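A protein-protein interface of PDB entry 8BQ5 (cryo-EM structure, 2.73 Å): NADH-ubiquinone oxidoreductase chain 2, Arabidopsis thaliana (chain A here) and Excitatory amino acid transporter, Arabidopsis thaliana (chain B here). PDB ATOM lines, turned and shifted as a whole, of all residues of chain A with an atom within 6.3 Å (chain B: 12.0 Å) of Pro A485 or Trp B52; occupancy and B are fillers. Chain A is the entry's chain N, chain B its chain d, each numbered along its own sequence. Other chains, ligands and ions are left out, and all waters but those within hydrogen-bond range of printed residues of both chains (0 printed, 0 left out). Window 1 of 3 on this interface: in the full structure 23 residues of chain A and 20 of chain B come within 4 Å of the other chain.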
ATOM      1  N   PHE A  95     -31.482  -0.890  31.755  1.00  0.00           N
ATOM      2  CA  PHE A  95     -30.193  -0.648  32.398  1.00  0.00           C
ATOM      3  C   PHE A  95     -30.208  -1.062  33.868  1.00  0.00           C
ATOM      4  O   PHE A  95     -29.201  -1.574  34.381  1.00  0.00           O
ATOM      5  CB  PHE A  95     -29.783   0.814  32.240  1.00  0.00           C
ATOM      6  CG  PHE A  95     -29.408   1.186  30.831  1.00  0.00           C
ATOM      7  CD1 PHE A  95     -28.326   0.583  30.209  1.00  0.00           C
ATOM      8  CD2 PHE A  95     -30.135   2.132  30.131  1.00  0.00           C
ATOM      9  CE1 PHE A  95     -27.977   0.919  28.916  1.00  0.00           C
ATOM     10  CE2 PHE A  95     -29.790   2.470  28.838  1.00  0.00           C
ATOM     11  CZ  PHE A  95     -28.710   1.862  28.229  1.00  0.00           C
ATOM     12  N   TYR A 482     -12.334   9.547  33.415  1.00  0.00           N
ATOM     13  CA  TYR A 482     -13.184   9.280  32.250  1.00  0.00           C
ATOM     14  C   TYR A 482     -14.580   8.861  32.706  1.00  0.00           C
ATOM     15  O   TYR A 482     -14.967   7.695  32.585  1.00  0.00           O
ATOM     16  CB  TYR A 482     -12.541   8.213  31.364  1.00  0.00           C
ATOM     17  CG  TYR A 482     -13.080   8.155  29.956  1.00  0.00           C
ATOM     18  CD1 TYR A 482     -14.171   7.359  29.644  1.00  0.00           C
ATOM     19  CD2 TYR A 482     -12.500   8.900  28.938  1.00  0.00           C
ATOM     20  CE1 TYR A 482     -14.667   7.299  28.359  1.00  0.00           C
ATOM     21  CE2 TYR A 482     -12.992   8.850  27.650  1.00  0.00           C
ATOM     22  CZ  TYR A 482     -14.076   8.047  27.367  1.00  0.00           C
ATOM     23  OH  TYR A 482     -14.574   7.988  26.086  1.00  0.00           O
ATOM     24  N   PRO A 483     -15.367   9.794  33.238  1.00  0.00           N
ATOM     25  CA  PRO A 483     -16.686   9.449  33.790  1.00  0.00           C
ATOM     26  C   PRO A 483     -17.862   9.590  32.833  1.00  0.00           C
ATOM     27  O   PRO A 483     -18.997   9.351  33.255  1.00  0.00           O
ATOM     28  CB  PRO A 483     -16.812  10.470  34.925  1.00  0.00           C
ATOM     29  CG  PRO A 483     -16.251  11.683  34.289  1.00  0.00           C
ATOM     30  CD  PRO A 483     -14.993  11.171  33.615  1.00  0.00           C
ATOM     31  N   SER A 484     -17.630   9.959  31.574  1.00  0.00           N
ATOM     32  CA  SER A 484     -18.729  10.315  30.676  1.00  0.00           C
ATOM     33  C   SER A 484     -19.756   9.206  30.464  1.00  0.00           C
ATOM     34  O   SER A 484     -20.962   9.518  30.450  1.00  0.00           O
ATOM     35  CB  SER A 484     -18.157  10.788  29.336  1.00  0.00           C
ATOM     36  OG  SER A 484     -19.162  11.399  28.550  1.00  0.00           O
ATOM     37  N   PRO A 485     -19.383   7.937  30.236  1.00  0.00           N
ATOM     38  CA  PRO A 485     -20.430   6.927  29.995  1.00  0.00           C
ATOM     39  C   PRO A 485     -21.438   6.805  31.125  1.00  0.00           C
ATOM     40  O   PRO A 485     -22.640   6.698  30.855  1.00  0.00           O
ATOM     41  CB  PRO A 485     -19.638   5.625  29.795  1.00  0.00           C
ATOM     42  CG  PRO A 485     -18.268   6.031  29.478  1.00  0.00           C
ATOM     43  CD  PRO A 485     -18.027   7.388  30.042  1.00  0.00           C
ATOM     44  N   LEU A 486     -20.991   6.846  32.383  1.00  0.00           N
ATOM     45  CA  LEU A 486     -21.932   6.760  33.496  1.00  0.00           C
ATOM     46  C   LEU A 486     -22.873   7.957  33.522  1.00  0.00           C
ATOM     47  O   LEU A 486     -24.086   7.798  33.707  1.00  0.00           O
ATOM     48  CB  LEU A 486     -21.186   6.652  34.826  1.00  0.00           C
ATOM     49  CG  LEU A 486     -22.120   6.392  36.011  1.00  0.00           C
ATOM     50  CD1 LEU A 486     -22.940   5.134  35.772  1.00  0.00           C
ATOM     51  CD2 LEU A 486     -21.366   6.316  37.330  1.00  0.00           C
ATOM     52  N   PHE A 487     -22.329   9.162  33.337  1.00  0.00           N
ATOM     53  CA  PHE A 487     -23.155  10.366  33.342  1.00  0.00           C
ATOM     54  C   PHE A 487     -24.215  10.301  32.251  1.00  0.00           C
ATOM     55  O   PHE A 487     -25.400  10.567  32.495  1.00  0.00           O
ATOM     56  CB  PHE A 487     -22.272  11.600  33.150  1.00  0.00           C
ATOM     57  CG  PHE A 487     -21.405  11.920  34.331  1.00  0.00           C
ATOM     58  CD1 PHE A 487     -21.593  11.286  35.547  1.00  0.00           C
ATOM     59  CD2 PHE A 487     -20.382  12.846  34.219  1.00  0.00           C
ATOM     60  CE1 PHE A 487     -20.792  11.581  36.629  1.00  0.00           C
ATOM     61  CE2 PHE A 487     -19.575  13.143  35.296  1.00  0.00           C
ATOM     62  CZ  PHE A 487     -19.780  12.510  36.503  1.00  0.00           C
ATOM     63  N   SER A 488     -23.805   9.921  31.040  1.00  0.00           N
ATOM     64  CA  SER A 488     -24.742   9.893  29.923  1.00  0.00           C
ATOM     65  C   SER A 488     -25.790   8.800  30.096  1.00  0.00           C
ATOM     66  O   SER A 488     -26.967   9.014  29.785  1.00  0.00           O
ATOM     67  CB  SER A 488     -23.985   9.711  28.610  1.00  0.00           C
ATOM     68  OG  SER A 488     -24.883   9.636  27.521  1.00  0.00           O
ATOM     69  N   VAL A 489     -25.395   7.623  30.589  1.00  0.00           N
ATOM     70  CA  VAL A 489     -26.363   6.539  30.719  1.00  0.00           C
ATOM     71  C   VAL A 489     -27.356   6.840  31.840  1.00  0.00           C
ATOM     72  O   VAL A 489     -28.552   6.536  31.727  1.00  0.00           O
ATOM     73  CB  VAL A 489     -25.643   5.188  30.912  1.00  0.00           C
ATOM     74  CG1 VAL A 489     -25.004   5.075  32.288  1.00  0.00           C
ATOM     75  CG2 VAL A 489     -26.596   4.035  30.650  1.00  0.00           C
ATOM     76  N   THR A 490     -26.894   7.473  32.922  1.00  0.00           N
ATOM     77  CA  THR A 490     -27.814   7.845  33.989  1.00  0.00           C
ATOM     78  C   THR A 490     -28.768   8.946  33.541  1.00  0.00           C
ATOM     79  O   THR A 490     -29.952   8.933  33.905  1.00  0.00           O
ATOM     80  CB  THR A 490     -27.035   8.271  35.232  1.00  0.00           C
ATOM     81  OG1 THR A 490     -25.966   9.146  34.852  1.00  0.00           O
ATOM     82  CG2 THR A 490     -26.464   7.049  35.937  1.00  0.00           C
ATOM     83  N   ALA B   5      -7.161   4.497  23.113  1.00  0.00           N
ATOM     84  CA  ALA B   5      -7.922   3.590  23.963  1.00  0.00           C
ATOM     85  C   ALA B   5      -7.264   2.222  24.050  1.00  0.00           C
ATOM     86  O   ALA B   5      -7.231   1.621  25.129  1.00  0.00           O
ATOM     87  CB  ALA B   5      -9.355   3.459  23.445  1.00  0.00           C
ATOM     88  N   ALA B  43      -7.510  -4.050  26.219  1.00  0.00           N
ATOM     89  CA  ALA B  43      -7.625  -3.319  24.959  1.00  0.00           C
ATOM     90  C   ALA B  43      -9.033  -3.440  24.379  1.00  0.00           C
ATOM     91  O   ALA B  43      -9.631  -2.443  23.936  1.00  0.00           O
ATOM     92  CB  ALA B  43      -6.583  -3.828  23.961  1.00  0.00           C
ATOM     93  N   VAL B  44      -9.582  -4.659  24.389  1.00  0.00           N
ATOM     94  CA  VAL B  44     -10.933  -4.867  23.871  1.00  0.00           C
ATOM     95  C   VAL B  44     -11.933  -4.029  24.660  1.00  0.00           C
ATOM     96  O   VAL B  44     -12.790  -3.341  24.088  1.00  0.00           O
ATOM     97  CB  VAL B  44     -11.297  -6.363  23.911  1.00  0.00           C
ATOM     98  CG1 VAL B  44     -12.809  -6.551  23.902  1.00  0.00           C
ATOM     99  CG2 VAL B  44     -10.649  -7.106  22.752  1.00  0.00           C
ATOM    100  N   PHE B  45     -11.816  -4.059  25.988  1.00  0.00           N
ATOM    101  CA  PHE B  45     -12.762  -3.359  26.847  1.00  0.00           C
ATOM    102  C   PHE B  45     -12.685  -1.851  26.647  1.00  0.00           C
ATOM    103  O   PHE B  45     -13.717  -1.174  26.628  1.00  0.00           O
ATOM    104  CB  PHE B  45     -12.499  -3.745  28.303  1.00  0.00           C
ATOM    105  CG  PHE B  45     -13.185  -2.868  29.310  1.00  0.00           C
ATOM    106  CD1 PHE B  45     -12.490  -1.871  29.969  1.00  0.00           C
ATOM    107  CD2 PHE B  45     -14.524  -3.056  29.610  1.00  0.00           C
ATOM    108  CE1 PHE B  45     -13.119  -1.076  30.904  1.00  0.00           C
ATOM    109  CE2 PHE B  45     -15.156  -2.260  30.542  1.00  0.00           C
ATOM    110  CZ  PHE B  45     -14.453  -1.268  31.190  1.00  0.00           C
ATOM    111  N   ALA B  46     -11.478  -1.305  26.482  1.00  0.00           N
ATOM    112  CA  ALA B  46     -11.354   0.138  26.289  1.00  0.00           C
ATOM    113  C   ALA B  46     -11.947   0.580  24.953  1.00  0.00           C
ATOM    114  O   ALA B  46     -12.668   1.591  24.890  1.00  0.00           O
ATOM    115  CB  ALA B  46      -9.891   0.558  26.398  1.00  0.00           C
ATOM    116  N   ASN B  47     -11.661  -0.159  23.874  1.00  0.00           N
ATOM    117  CA  ASN B  47     -12.248   0.210  22.589  1.00  0.00           C
ATOM    118  C   ASN B  47     -13.769   0.127  22.638  1.00  0.00           C
ATOM    119  O   ASN B  47     -14.469   1.039  22.168  1.00  0.00           O
ATOM    120  CB  ASN B  47     -11.691  -0.677  21.476  1.00  0.00           C
ATOM    121  CG  ASN B  47     -10.351  -0.193  20.967  1.00  0.00           C
ATOM    122  OD1 ASN B  47     -10.093   1.009  20.912  1.00  0.00           O
ATOM    123  ND2 ASN B  47      -9.485  -1.128  20.596  1.00  0.00           N
ATOM    124  N   GLN B  48     -14.300  -0.941  23.240  1.00  0.00           N
ATOM    125  CA  GLN B  48     -15.747  -1.075  23.353  1.00  0.00           C
ATOM    126  C   GLN B  48     -16.343   0.046  24.194  1.00  0.00           C
ATOM    127  O   GLN B  48     -17.427   0.546  23.885  1.00  0.00           O
ATOM    128  CB  GLN B  48     -16.105  -2.441  23.939  1.00  0.00           C
ATOM    129  CG  GLN B  48     -15.826  -3.609  23.004  1.00  0.00           C
ATOM    130  CD  GLN B  48     -16.562  -3.502  21.681  1.00  0.00           C
ATOM    131  OE1 GLN B  48     -17.577  -2.811  21.569  1.00  0.00           O
ATOM    132  NE2 GLN B  48     -16.045  -4.179  20.665  1.00  0.00           N
ATOM    133  N   LEU B  49     -15.650   0.451  25.262  1.00  0.00           N
ATOM    134  CA  LEU B  49     -16.167   1.515  26.115  1.00  0.00           C
ATOM    135  C   LEU B  49     -16.247   2.840  25.370  1.00  0.00           C
ATOM    136  O   LEU B  49     -17.227   3.580  25.515  1.00  0.00           O
ATOM    137  CB  LEU B  49     -15.301   1.660  27.364  1.00  0.00           C
ATOM    138  CG  LEU B  49     -15.883   2.576  28.443  1.00  0.00           C
ATOM    139  CD1 LEU B  49     -17.030   1.902  29.183  1.00  0.00           C
ATOM    140  CD2 LEU B  49     -14.804   3.030  29.409  1.00  0.00           C
ATOM    141  N   VAL B  50     -15.227   3.163  24.574  1.00  0.00           N
ATOM    142  CA  VAL B  50     -15.265   4.417  23.819  1.00  0.00           C
ATOM    143  C   VAL B  50     -16.407   4.391  22.804  1.00  0.00           C
ATOM    144  O   VAL B  50     -17.178   5.358  22.674  1.00  0.00           O
ATOM    145  CB  VAL B  50     -13.908   4.683  23.145  1.00  0.00           C
ATOM    146  CG1 VAL B  50     -14.036   5.784  22.112  1.00  0.00           C
ATOM    147  CG2 VAL B  50     -12.880   5.066  24.191  1.00  0.00           C
ATOM    148  N   LYS B  51     -16.547   3.271  22.086  1.00  0.00           N
ATOM    149  CA  LYS B  51     -17.643   3.154  21.125  1.00  0.00           C
ATOM    150  C   LYS B  51     -19.002   3.285  21.811  1.00  0.00           C
ATOM    151  O   LYS B  51     -19.905   3.975  21.311  1.00  0.00           O
ATOM    152  CB  LYS B  51     -17.542   1.818  20.392  1.00  0.00           C
ATOM    153  CG  LYS B  51     -16.174   1.533  19.801  1.00  0.00           C
ATOM    154  CD  LYS B  51     -16.293   0.940  18.421  1.00  0.00           C
ATOM    155  CE  LYS B  51     -15.552  -0.382  18.329  1.00  0.00           C
ATOM    156  NZ  LYS B  51     -14.195  -0.219  17.747  1.00  0.00           N
ATOM    157  N   TRP B  52     -19.158   2.637  22.966  1.00  0.00           N
ATOM    158  CA  TRP B  52     -20.412   2.698  23.704  1.00  0.00           C
ATOM    159  C   TRP B  52     -20.709   4.113  24.177  1.00  0.00           C
ATOM    160  O   TRP B  52     -21.865   4.544  24.167  1.00  0.00           O
ATOM    161  CB  TRP B  52     -20.362   1.739  24.891  1.00  0.00           C
ATOM    162  CG  TRP B  52     -21.642   1.650  25.647  1.00  0.00           C
ATOM    163  CD1 TRP B  52     -22.877   1.382  25.138  1.00  0.00           C
ATOM    164  CD2 TRP B  52     -21.818   1.832  27.055  1.00  0.00           C
ATOM    165  NE1 TRP B  52     -23.812   1.380  26.142  1.00  0.00           N
ATOM    166  CE2 TRP B  52     -23.187   1.655  27.330  1.00  0.00           C
ATOM    167  CE3 TRP B  52     -20.950   2.125  28.110  1.00  0.00           C
ATOM    168  CZ2 TRP B  52     -23.708   1.762  28.616  1.00  0.00           C
ATOM    169  CZ3 TRP B  52     -21.469   2.232  29.384  1.00  0.00           C
ATOM    170  CH2 TRP B  52     -22.836   2.052  29.627  1.00  0.00           C
ATOM    171  N   ASP B  53     -19.682   4.844  24.615  1.00  0.00           N
ATOM    172  CA  ASP B  53     -19.884   6.234  25.015  1.00  0.00           C
ATOM    173  C   ASP B  53     -20.400   7.065  23.848  1.00  0.00           C
ATOM    174  O   ASP B  53     -21.312   7.890  24.013  1.00  0.00           O
ATOM    175  CB  ASP B  53     -18.577   6.816  25.556  1.00  0.00           C
ATOM    176  CG  ASP B  53     -18.787   8.090  26.360  1.00  0.00           C
ATOM    177  OD1 ASP B  53     -19.929   8.595  26.409  1.00  0.00           O
ATOM    178  OD2 ASP B  53     -17.801   8.593  26.937  1.00  0.00           O
ATOM    179  N   VAL B  54     -19.833   6.859  22.655  1.00  0.00           N
ATOM    180  CA  VAL B  54     -20.306   7.603  21.486  1.00  0.00           C
ATOM    181  C   VAL B  54     -21.778   7.297  21.222  1.00  0.00           C
ATOM    182  O   VAL B  54     -22.598   8.205  21.007  1.00  0.00           O
ATOM    183  CB  VAL B  54     -19.433   7.292  20.257  1.00  0.00           C
ATOM    184  CG1 VAL B  54     -20.011   7.954  19.017  1.00  0.00           C
ATOM    185  CG2 VAL B  54     -18.010   7.758  20.493  1.00  0.00           C
ATOM    186  N   LYS B  55     -22.136   6.011  21.257  1.00  0.00           N
ATOM    187  CA  LYS B  55     -23.525   5.627  21.007  1.00  0.00           C
ATOM    188  C   LYS B  55     -24.465   6.217  22.057  1.00  0.00           C
ATOM    189  O   LYS B  55     -25.570   6.676  21.730  1.00  0.00           O
ATOM    190  CB  LYS B  55     -23.648   4.105  20.977  1.00  0.00           C
ATOM    191  CG  LYS B  55     -25.041   3.602  20.652  1.00  0.00           C
ATOM    192  CD  LYS B  55     -25.071   2.085  20.594  1.00  0.00           C
ATOM    193  CE  LYS B  55     -26.470   1.570  20.292  1.00  0.00           C
ATOM    194  NZ  LYS B  55     -26.516   0.081  20.231  1.00  0.00           N
ATOM    195  N   LEU B  56     -24.048   6.199  23.325  1.00  0.00           N
ATOM    196  CA  LEU B  56     -24.877   6.738  24.396  1.00  0.00           C
ATOM    197  C   LEU B  56     -25.123   8.225  24.212  1.00  0.00           C
ATOM    198  O   LEU B  56     -26.244   8.704  24.420  1.00  0.00           O
ATOM    199  CB  LEU B  56     -24.220   6.488  25.751  1.00  0.00           C
ATOM    200  CG  LEU B  56     -24.199   5.092  26.362  1.00  0.00           C
ATOM    201  CD1 LEU B  56     -23.322   5.114  27.600  1.00  0.00           C
ATOM    202  CD2 LEU B  56     -25.605   4.639  26.711  1.00  0.00           C
ATOM    203  N   LYS B  57     -24.082   8.980  23.852  1.00  0.00           N
ATOM    204  CA  LYS B  57     -24.274  10.406  23.604  1.00  0.00           C
ATOM    205  C   LYS B  57     -25.233  10.627  22.442  1.00  0.00           C
ATOM    206  O   LYS B  57     -26.104  11.508  22.500  1.00  0.00           O
ATOM    207  CB  LYS B  57     -22.928  11.082  23.344  1.00  0.00           C
ATOM    208  CG  LYS B  57     -22.521  12.090  24.422  1.00  0.00           C
ATOM    209  CD  LYS B  57     -21.115  12.616  24.174  1.00  0.00           C
ATOM    210  CE  LYS B  57     -20.156  12.023  25.180  1.00  0.00           C
ATOM    211  NZ  LYS B  57     -18.802  12.165  24.738  1.00  0.00           N
ATOM    212  N   GLU B  58     -25.103   9.815  21.389  1.00  0.00           N
ATOM    213  CA  GLU B  58     -26.011   9.935  20.254  1.00  0.00           C
ATOM    214  C   GLU B  58     -27.459   9.719  20.675  1.00  0.00           C
ATOM    215  O   GLU B  58     -28.356  10.454  20.246  1.00  0.00           O
ATOM    216  CB  GLU B  58     -25.621   8.937  19.168  1.00  0.00           C
ATOM    217  CG  GLU B  58     -25.921   9.411  17.765  1.00  0.00           C
ATOM    218  CD  GLU B  58     -24.977   8.814  16.747  1.00  0.00           C
ATOM    219  OE1 GLU B  58     -24.814   9.409  15.662  1.00  0.00           O
ATOM    220  OE2 GLU B  58     -24.399   7.745  17.033  1.00  0.00           O
ATOM    221  N   ASP B  59     -27.709   8.711  21.511  1.00  0.00           N
ATOM    222  CA  ASP B  59     -29.077   8.432  21.945  1.00  0.00           C
ATOM    223  C   ASP B  59     -29.606   9.526  22.872  1.00  0.00           C
ATOM    224  O   ASP B  59     -30.774   9.939  22.768  1.00  0.00           O
ATOM    225  CB  ASP B  59     -29.129   7.066  22.625  1.00  0.00           C
ATOM    226  CG  ASP B  59     -28.764   5.939  21.680  1.00  0.00           C
ATOM    227  OD1 ASP B  59     -29.043   6.069  20.470  1.00  0.00           O
ATOM    228  OD2 ASP B  59     -28.195   4.927  22.142  1.00  0.00           O
ATOM    229  N   LEU B  60     -28.759  10.001  23.789  1.00  0.00           N
ATOM    230  CA  LEU B  60     -29.160  11.066  24.697  1.00  0.00           C
ATOM    231  C   LEU B  60     -29.531  12.333  23.943  1.00  0.00           C
ATOM    232  O   LEU B  60     -30.430  13.063  24.372  1.00  0.00           O
ATOM    233  CB  LEU B  60     -28.042  11.354  25.699  1.00  0.00           C
ATOM    234  CG  LEU B  60     -28.378  12.377  26.786  1.00  0.00           C
ATOM    235  CD1 LEU B  60     -29.552  11.916  27.635  1.00  0.00           C
ATOM    236  CD2 LEU B  60     -27.165  12.677  27.653  1.00  0.00           C
ATOM    237  N   ASP B  61     -28.854  12.617  22.830  1.00  0.00           N
ATOM    238  CA  ASP B  61     -29.192  13.813  22.063  1.00  0.00           C
ATOM    239  C   ASP B  61     -30.623  13.747  21.537  1.00  0.00           C
ATOM    240  O   ASP B  61     -31.387  14.713  21.652  1.00  0.00           O
ATOM    241  CB  ASP B  61     -28.196  14.001  20.920  1.00  0.00           C
ATOM    242  CG  ASP B  61     -26.830  14.438  21.409  1.00  0.00           C
ATOM    243  OD1 ASP B  61     -26.708  14.776  22.604  1.00  0.00           O
ATOM    244  OD2 ASP B  61     -25.879  14.439  20.601  1.00  0.00           O
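Of the 10 printed residues of chain A, 4 touch a printed residue of chain B. Hydrophobic or aromatic side chains of chain A that line the printed part of chain B: Tyr A482 and Pro A485.
The side-chain hydroxyl of Tyr A482 lies within hydrogen-bond range of the side-chain carboxylate of Asp B53 (3.4 Å).
Among the printed residues, pairs that only touch across the chains: Ser A484 with Asp B53, Pro A485 with Asp B53, Ser A488 with Leu B56, Ser A484 with Lys B57, Pro A485 with Leu B56, Ser A488 with Leu B60, Ser A488 with Lys B57, Tyr A482 with Val B50 and Pro A485 with Trp B52.
Of chain B, only Trp B52, Asp B53 and Leu B56 come within 4 Å of Pro A485. No residue of chain B comes within 4 Å of Pro A483. Ser A484 touches just these residues of chain B: Asp B53 (3.3 Å) and Lys B57 (3.6 Å). Phe A487 touches none of the printed residues of chain B. Val A489 touches none of the printed residues of chain B. Of the printed residues of chain A, Asp B53 touches Tyr A482 (3.4 Å), Ser A484 (3.3 Å) and Pro A485 (3.3 Å). Of the printed residues of chain A, Val B50 touches Tyr A482. Printed residues of chain A within 4 Å of Leu B60: Ser A488. Gln B48 touches none of the printed residues of chain A. The nearest residue of chain B that does not touch Pro A485 is Leu B49 (4.3 Å). The nearest residue of chain A that does not touch Trp B52 is Val A489 (4.2 Å).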
